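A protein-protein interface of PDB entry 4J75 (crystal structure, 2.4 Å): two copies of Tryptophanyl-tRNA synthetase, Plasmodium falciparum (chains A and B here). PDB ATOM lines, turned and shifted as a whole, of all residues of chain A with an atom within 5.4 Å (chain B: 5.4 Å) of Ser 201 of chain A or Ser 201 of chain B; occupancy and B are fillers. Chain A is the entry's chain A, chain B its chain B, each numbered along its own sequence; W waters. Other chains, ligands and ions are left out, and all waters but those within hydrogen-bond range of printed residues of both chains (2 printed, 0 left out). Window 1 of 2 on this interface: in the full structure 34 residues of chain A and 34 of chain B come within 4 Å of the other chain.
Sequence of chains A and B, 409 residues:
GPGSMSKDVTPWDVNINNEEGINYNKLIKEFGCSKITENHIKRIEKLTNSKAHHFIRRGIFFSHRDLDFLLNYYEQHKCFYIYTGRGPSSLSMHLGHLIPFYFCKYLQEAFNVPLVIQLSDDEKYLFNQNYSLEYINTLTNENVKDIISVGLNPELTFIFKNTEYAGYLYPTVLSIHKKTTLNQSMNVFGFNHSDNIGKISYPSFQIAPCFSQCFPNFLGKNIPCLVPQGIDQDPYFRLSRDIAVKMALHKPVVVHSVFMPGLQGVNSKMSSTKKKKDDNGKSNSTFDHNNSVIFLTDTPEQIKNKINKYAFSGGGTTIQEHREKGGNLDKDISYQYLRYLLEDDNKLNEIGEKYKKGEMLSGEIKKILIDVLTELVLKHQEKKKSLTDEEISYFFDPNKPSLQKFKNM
The backbone carbonyl oxygen (O) of Ile 197 of chain A lies close to the side-chain hydroxyl (OG) of Ser 201 of chain A, 3.4 Å away.
O of Ile 197 of chain B sits close to OG of Ser 201 of chain B.
The backbone carbonyl oxygen of Gly 198 of chain B sits at hydrogen-bond distance from the side-chain hydroxyl of Ser 201 of chain B (3.3 Å).
OG of Ser 185 of chain B lies within hydrogen-bond range of O of Ile 200 of chain B (3.2 Å).
The side-chain hydroxyl of Ser 185 of chain A lies within hydrogen-bond range of the backbone carbonyl oxygen of Ile 200 of chain A.
A ring nitrogen (ND1) of His 177 of chain A lies within hydrogen-bond range of the side-chain hydroxyl (OG) of Ser 204 of chain A (2.8 Å).
Among the printed residues, pairs that only touch across the chains: His 177 of chain A with Ile 197 of chain B, His 177 of chain A with Gly 198 of chain B, His 177 of chain A with Ser 201 of chain B, Ser 185 of chain A with Ile 197 of chain B, Ile 197 of chain A with His 177 of chain B, Ile 197 of chain A with Ser 185 of chain B, Ile 197 of chain A with Ile 200 of chain B, Ile 197 of chain A with Ser 204 of chain B, Gly 198 of chain A with His 177 of chain B, Ile 200 of chain A with Ile 197 of chain B, Ser 201 of chain A with His 177 of chain B, Ser 201 of chain A with Ser 201 of chain B and Ser 204 of chain A with Ile 197 of chain B.
Of chain B, only His 177 (3.9 Å) and Ser 201 (3.8 Å) come within 4 Å of Ser 201 of chain A.
Of the printed residues of chain B, Gly 198 of chain A touches His 177.
Of the printed residues of chain B, Ile 197 of chain A touches His 177 (3.5 Å), Ser 185 (3.8 Å), Ile 200 (3.7 Å) and Ser 204 (3.5 Å).
Of the printed residues of chain B, Ser 185 of chain A touches Ile 197 (3.8 Å).
Of the printed residues of chain B, Ile 200 of chain A touches Ile 197.
Of the printed residues of chain A, Ile 200 of chain B touches Ile 197.
The nearest residue of chain B that does not touch Ser 201 of chain A is Ile 197 of chain B (4.4 Å).
The nearest printed residue of chain B that does not touch Ile 197 of chain A is Ser 201 of chain B (4.3 Å).
Printed residues of chain B that touch a printed residue of chain A: His 177, Ser 185, Ile 197, Gly 198, Ile 200, Ser 201 and Ser 204.
Hydrophobic or aromatic side chains of chain A that line the printed part of chain B: His 177, Ile 197 and Ile 200.
Along chain A the printed residues that touch a printed residue of chain B span positions 177 to 204.
Among the printed residues, 13 pairs touch across the chains.
His 177 of chain A touches Gly 198 of chain B, and with the chains exchanged Gly 198 of chain A touches His 177 of chain B.
His 177 of chain A touches Ser 201 of chain B, and with the chains exchanged Ser 201 of chain A touches His 177 of chain B.
Ser 185 of chain A touches Ile 197 of chain B, and with the chains exchanged Ile 197 of chain A touches Ser 185 of chain B.
Ile 197 of chain A touches Ser 204 of chain B, and with the chains exchanged Ser 204 of chain A touches Ile 197 of chain B.
Water W1 lies within hydrogen-bond range of OG of Ser 201 of chain B (2.7 Å) and NE2 of His 177 of chain A (2.8 Å).
Water W2 bridges NE2 of His 177 of chain B (2.9 Å) and OG of Ser 201 of chain A (3.1 Å).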
ATOM      1  N   HIS A 177      -1.517  17.447   8.906  1.00  0.00           N
ATOM      2  CA  HIS A 177      -1.372  18.660   8.098  1.00  0.00           C
ATOM      3  C   HIS A 177      -2.568  19.570   8.278  1.00  0.00           C
ATOM      4  O   HIS A 177      -2.407  20.767   8.534  1.00  0.00           O
ATOM      5  CB  HIS A 177      -1.288  18.349   6.594  1.00  0.00           C
ATOM      6  CG  HIS A 177       0.065  17.939   6.107  1.00  0.00           C
ATOM      7  ND1 HIS A 177       1.215  18.074   6.854  1.00  0.00           N
ATOM      8  CD2 HIS A 177       0.448  17.417   4.916  1.00  0.00           C
ATOM      9  CE1 HIS A 177       2.243  17.635   6.150  1.00  0.00           C
ATOM     10  NE2 HIS A 177       1.804  17.240   4.968  1.00  0.00           N
ATOM     11  N   SER A 185       3.262  25.961  12.486  1.00  0.00           N
ATOM     12  CA  SER A 185       4.464  25.266  12.020  1.00  0.00           C
ATOM     13  C   SER A 185       5.658  26.218  12.147  1.00  0.00           C
ATOM     14  O   SER A 185       6.673  25.871  12.741  1.00  0.00           O
ATOM     15  CB  SER A 185       4.278  24.795  10.572  1.00  0.00           C
ATOM     16  OG  SER A 185       5.433  24.146  10.054  1.00  0.00           O
ATOM     17  N   ILE A 197       9.219  24.247   1.194  1.00  0.00           N
ATOM     18  CA  ILE A 197       7.948  23.757   1.738  1.00  0.00           C
ATOM     19  C   ILE A 197       8.029  22.319   2.243  1.00  0.00           C
ATOM     20  O   ILE A 197       7.156  21.876   2.985  1.00  0.00           O
ATOM     21  CB  ILE A 197       6.798  23.884   0.718  1.00  0.00           C
ATOM     22  CG1 ILE A 197       7.067  23.044  -0.538  1.00  0.00           C
ATOM     23  CG2 ILE A 197       6.584  25.352   0.361  1.00  0.00           C
ATOM     24  CD1 ILE A 197       5.928  23.081  -1.541  1.00  0.00           C
ATOM     25  N   GLY A 198       9.068  21.597   1.842  1.00  0.00           N
ATOM     26  CA  GLY A 198       9.352  20.296   2.424  1.00  0.00           C
ATOM     27  C   GLY A 198       9.652  20.363   3.915  1.00  0.00           C
ATOM     28  O   GLY A 198       9.160  19.542   4.694  1.00  0.00           O
ATOM     29  N   LYS A 199      10.470  21.334   4.303  1.00  0.00           N
ATOM     30  CA  LYS A 199      10.772  21.574   5.709  1.00  0.00           C
ATOM     31  C   LYS A 199       9.508  21.910   6.476  1.00  0.00           C
ATOM     32  O   LYS A 199       9.252  21.343   7.531  1.00  0.00           O
ATOM     33  CB  LYS A 199      11.773  22.718   5.863  1.00  0.00           C
ATOM     34  CG  LYS A 199      13.132  22.396   5.294  1.00  0.00           C
ATOM     35  CD  LYS A 199      14.243  23.145   5.994  1.00  0.00           C
ATOM     36  CE  LYS A 199      14.718  24.301   5.174  1.00  0.00           C
ATOM     37  NZ  LYS A 199      15.890  24.926   5.839  1.00  0.00           N
ATOM     38  N   ILE A 200       8.715  22.831   5.939  1.00  0.00           N
ATOM     39  CA  ILE A 200       7.456  23.215   6.582  1.00  0.00           C
ATOM     40  C   ILE A 200       6.610  21.977   6.844  1.00  0.00           C
ATOM     41  O   ILE A 200       5.956  21.875   7.881  1.00  0.00           O
ATOM     42  CB  ILE A 200       6.624  24.178   5.724  1.00  0.00           C
ATOM     43  CG1 ILE A 200       7.417  25.439   5.334  1.00  0.00           C
ATOM     44  CG2 ILE A 200       5.329  24.551   6.436  1.00  0.00           C
ATOM     45  CD1 ILE A 200       8.098  26.150   6.459  1.00  0.00           C
ATOM     46  N   SER A 201       6.622  21.041   5.896  1.00  0.00           N
ATOM     47  CA  SER A 201       5.697  19.925   5.921  1.00  0.00           C
ATOM     48  C   SER A 201       6.246  18.661   6.603  1.00  0.00           C
ATOM     49  O   SER A 201       5.473  17.826   7.025  1.00  0.00           O
ATOM     50  CB  SER A 201       5.208  19.626   4.500  1.00  0.00           C
ATOM     51  OG  SER A 201       6.067  18.739   3.810  1.00  0.00           O
ATOM     52  N   TYR A 202       7.562  18.543   6.753  1.00  0.00           N
ATOM     53  CA  TYR A 202       8.157  17.359   7.390  1.00  0.00           C
ATOM     54  C   TYR A 202       7.633  16.969   8.793  1.00  0.00           C
ATOM     55  O   TYR A 202       7.440  15.792   9.063  1.00  0.00           O
ATOM     56  CB  TYR A 202       9.693  17.448   7.462  1.00  0.00           C
ATOM     57  CG  TYR A 202      10.215  16.353   8.356  1.00  0.00           C
ATOM     58  CD1 TYR A 202      10.203  15.037   7.930  1.00  0.00           C
ATOM     59  CD2 TYR A 202      10.626  16.623   9.654  1.00  0.00           C
ATOM     60  CE1 TYR A 202      10.615  14.008   8.757  1.00  0.00           C
ATOM     61  CE2 TYR A 202      11.041  15.608  10.492  1.00  0.00           C
ATOM     62  CZ  TYR A 202      11.035  14.296  10.034  1.00  0.00           C
ATOM     63  OH  TYR A 202      11.443  13.261  10.847  1.00  0.00           O
ATOM     64  N   PRO A 203       7.429  17.934   9.700  1.00  0.00           N
ATOM     65  CA  PRO A 203       7.056  17.530  11.071  1.00  0.00           C
ATOM     66  C   PRO A 203       5.864  16.595  11.187  1.00  0.00           C
ATOM     67  O   PRO A 203       5.830  15.782  12.102  1.00  0.00           O
ATOM     68  CB  PRO A 203       6.741  18.866  11.752  1.00  0.00           C
ATOM     69  CG  PRO A 203       7.636  19.826  11.063  1.00  0.00           C
ATOM     70  CD  PRO A 203       7.642  19.385   9.617  1.00  0.00           C
ATOM     71  N   SER A 204       4.900  16.703  10.276  1.00  0.00           N
ATOM     72  CA  SER A 204       3.750  15.808  10.262  1.00  0.00           C
ATOM     73  C   SER A 204       4.190  14.367  10.009  1.00  0.00           C
ATOM     74  O   SER A 204       3.586  13.427  10.545  1.00  0.00           O
ATOM     75  CB  SER A 204       2.734  16.244   9.194  1.00  0.00           C
ATOM     76  OG  SER A 204       2.290  17.579   9.419  1.00  0.00           O
ATOM     77  N   PHE A 205       5.243  14.201   9.210  1.00  0.00           N
ATOM     78  CA  PHE A 205       5.809  12.886   8.945  1.00  0.00           C
ATOM     79  C   PHE A 205       6.508  12.302  10.178  1.00  0.00           C
ATOM     80  O   PHE A 205       6.452  11.085  10.398  1.00  0.00           O
ATOM     81  CB  PHE A 205       6.772  12.925   7.757  1.00  0.00           C
ATOM     82  CG  PHE A 205       6.079  13.049   6.425  1.00  0.00           C
ATOM     83  CD1 PHE A 205       5.672  14.283   5.958  1.00  0.00           C
ATOM     84  CD2 PHE A 205       5.824  11.934   5.649  1.00  0.00           C
ATOM     85  CE1 PHE A 205       5.032  14.406   4.737  1.00  0.00           C
ATOM     86  CE2 PHE A 205       5.186  12.049   4.422  1.00  0.00           C
ATOM     87  CZ  PHE A 205       4.788  13.292   3.965  1.00  0.00           C
ATOM     88  N   HIS B 177       9.472  19.778  -3.541  1.00  0.00           N
ATOM     89  CA  HIS B 177       9.443  20.514  -2.276  1.00  0.00           C
ATOM     90  C   HIS B 177      10.722  21.304  -2.077  1.00  0.00           C
ATOM     91  O   HIS B 177      10.681  22.505  -1.770  1.00  0.00           O
ATOM     92  CB  HIS B 177       9.303  19.579  -1.063  1.00  0.00           C
ATOM     93  CG  HIS B 177       7.906  19.102  -0.782  1.00  0.00           C
ATOM     94  ND1 HIS B 177       6.784  19.655  -1.354  1.00  0.00           N
ATOM     95  CD2 HIS B 177       7.458  18.122   0.041  1.00  0.00           C
ATOM     96  CE1 HIS B 177       5.709  19.021  -0.919  1.00  0.00           C
ATOM     97  NE2 HIS B 177       6.089  18.095  -0.060  1.00  0.00           N
ATOM     98  N   SER B 185       5.517  29.319  -3.015  1.00  0.00           N
ATOM     99  CA  SER B 185       4.264  28.598  -2.870  1.00  0.00           C
ATOM    100  C   SER B 185       3.144  29.587  -2.561  1.00  0.00           C
ATOM    101  O   SER B 185       2.124  29.625  -3.264  1.00  0.00           O
ATOM    102  CB  SER B 185       4.376  27.544  -1.765  1.00  0.00           C
ATOM    103  OG  SER B 185       3.161  26.842  -1.558  1.00  0.00           O
ATOM    104  N   ILE B 197      -0.767  23.492   6.515  1.00  0.00           N
ATOM    105  CA  ILE B 197       0.471  23.192   5.803  1.00  0.00           C
ATOM    106  C   ILE B 197       0.272  22.126   4.729  1.00  0.00           C
ATOM    107  O   ILE B 197       1.125  21.961   3.850  1.00  0.00           O
ATOM    108  CB  ILE B 197       1.599  22.773   6.760  1.00  0.00           C
ATOM    109  CG1 ILE B 197       1.229  21.509   7.548  1.00  0.00           C
ATOM    110  CG2 ILE B 197       1.928  23.922   7.703  1.00  0.00           C
ATOM    111  CD1 ILE B 197       2.334  21.016   8.465  1.00  0.00           C
ATOM    112  N   GLY B 198      -0.844  21.410   4.797  1.00  0.00           N
ATOM    113  CA  GLY B 198      -1.225  20.500   3.725  1.00  0.00           C
ATOM    114  C   GLY B 198      -1.490  21.213   2.413  1.00  0.00           C
ATOM    115  O   GLY B 198      -1.047  20.763   1.363  1.00  0.00           O
ATOM    116  N   LYS B 199      -2.216  22.321   2.488  1.00  0.00           N
ATOM    117  CA  LYS B 199      -2.469  23.177   1.335  1.00  0.00           C
ATOM    118  C   LYS B 199      -1.159  23.705   0.767  1.00  0.00           C
ATOM    119  O   LYS B 199      -0.912  23.611  -0.425  1.00  0.00           O
ATOM    120  CB  LYS B 199      -3.363  24.354   1.711  1.00  0.00           C
ATOM    121  CG  LYS B 199      -4.755  23.978   2.178  1.00  0.00           C
ATOM    122  CD  LYS B 199      -5.619  25.212   2.483  1.00  0.00           C
ATOM    123  CE  LYS B 199      -6.159  25.961   1.283  1.00  0.00           C
ATOM    124  NZ  LYS B 199      -6.997  27.124   1.726  1.00  0.00           N
ATOM    125  N   ILE B 200      -0.301  24.226   1.631  1.00  0.00           N
ATOM    126  CA  ILE B 200       1.006  24.723   1.197  1.00  0.00           C
ATOM    127  C   ILE B 200       1.776  23.642   0.428  1.00  0.00           C
ATOM    128  O   ILE B 200       2.442  23.931  -0.555  1.00  0.00           O
ATOM    129  CB  ILE B 200       1.886  25.154   2.387  1.00  0.00           C
ATOM    130  CG1 ILE B 200       1.186  26.186   3.280  1.00  0.00           C
ATOM    131  CG2 ILE B 200       3.221  25.679   1.896  1.00  0.00           C
ATOM    132  CD1 ILE B 200       0.590  27.369   2.572  1.00  0.00           C
ATOM    133  N   SER B 201       1.662  22.395   0.881  1.00  0.00           N
ATOM    134  CA  SER B 201       2.485  21.321   0.363  1.00  0.00           C
ATOM    135  C   SER B 201       1.845  20.537  -0.782  1.00  0.00           C
ATOM    136  O   SER B 201       2.551  19.895  -1.537  1.00  0.00           O
ATOM    137  CB  SER B 201       2.907  20.390   1.515  1.00  0.00           C
ATOM    138  OG  SER B 201       1.953  19.371   1.769  1.00  0.00           O
ATOM    139  N   TYR B 202       0.523  20.605  -0.938  1.00  0.00           N
ATOM    140  CA  TYR B 202      -0.163  19.863  -2.005  1.00  0.00           C
ATOM    141  C   TYR B 202       0.367  20.067  -3.442  1.00  0.00           C
ATOM    142  O   TYR B 202       0.443  19.111  -4.205  1.00  0.00           O
ATOM    143  CB  TYR B 202      -1.692  20.127  -2.005  1.00  0.00           C
ATOM    144  CG  TYR B 202      -2.298  19.594  -3.271  1.00  0.00           C
ATOM    145  CD1 TYR B 202      -2.404  18.225  -3.477  1.00  0.00           C
ATOM    146  CD2 TYR B 202      -2.655  20.442  -4.307  1.00  0.00           C
ATOM    147  CE1 TYR B 202      -2.887  17.717  -4.667  1.00  0.00           C
ATOM    148  CE2 TYR B 202      -3.153  19.943  -5.494  1.00  0.00           C
ATOM    149  CZ  TYR B 202      -3.263  18.576  -5.669  1.00  0.00           C
ATOM    150  OH  TYR B 202      -3.747  18.068  -6.841  1.00  0.00           O
ATOM    151  N   PRO B 203       0.687  21.308  -3.844  1.00  0.00           N
ATOM    152  CA  PRO B 203       1.018  21.500  -5.259  1.00  0.00           C
ATOM    153  C   PRO B 203       2.113  20.587  -5.803  1.00  0.00           C
ATOM    154  O   PRO B 203       2.099  20.278  -6.987  1.00  0.00           O
ATOM    155  CB  PRO B 203       1.473  22.960  -5.313  1.00  0.00           C
ATOM    156  CG  PRO B 203       0.648  23.605  -4.257  1.00  0.00           C
ATOM    157  CD  PRO B 203       0.574  22.594  -3.142  1.00  0.00           C
ATOM    158  N   SER B 204       3.063  20.200  -4.956  1.00  0.00           N
ATOM    159  CA  SER B 204       4.141  19.325  -5.377  1.00  0.00           C
ATOM    160  C   SER B 204       3.567  17.955  -5.786  1.00  0.00           C
ATOM    161  O   SER B 204       4.086  17.300  -6.694  1.00  0.00           O
ATOM    162  CB  SER B 204       5.164  19.178  -4.259  1.00  0.00           C
ATOM    163  OG  SER B 204       5.722  20.435  -3.879  1.00  0.00           O
ATOM    164  N   PHE B 205       2.481  17.551  -5.122  1.00  0.00           N
ATOM    165  CA  PHE B 205       1.802  16.305  -5.443  1.00  0.00           C
ATOM    166  C   PHE B 205       1.089  16.399  -6.791  1.00  0.00           C
ATOM    167  O   PHE B 205       1.017  15.406  -7.524  1.00  0.00           O
ATOM    168  CB  PHE B 205       0.816  15.910  -4.329  1.00  0.00           C
ATOM    169  CG  PHE B 205       1.486  15.386  -3.092  1.00  0.00           C
ATOM    170  CD1 PHE B 205       1.995  16.255  -2.138  1.00  0.00           C
ATOM    171  CD2 PHE B 205       1.625  14.024  -2.893  1.00  0.00           C
ATOM    172  CE1 PHE B 205       2.628  15.775  -1.006  1.00  0.00           C
ATOM    173  CE2 PHE B 205       2.253  13.540  -1.762  1.00  0.00           C
ATOM    174  CZ  PHE B 205       2.759  14.416  -0.818  1.00  0.00           C
HETATM  175  O   HOH W   1       2.633  16.816   2.365  1.00  0.00           O
HETATM  176  O   HOH W   2       5.239  16.299   2.064  1.00  0.00           O
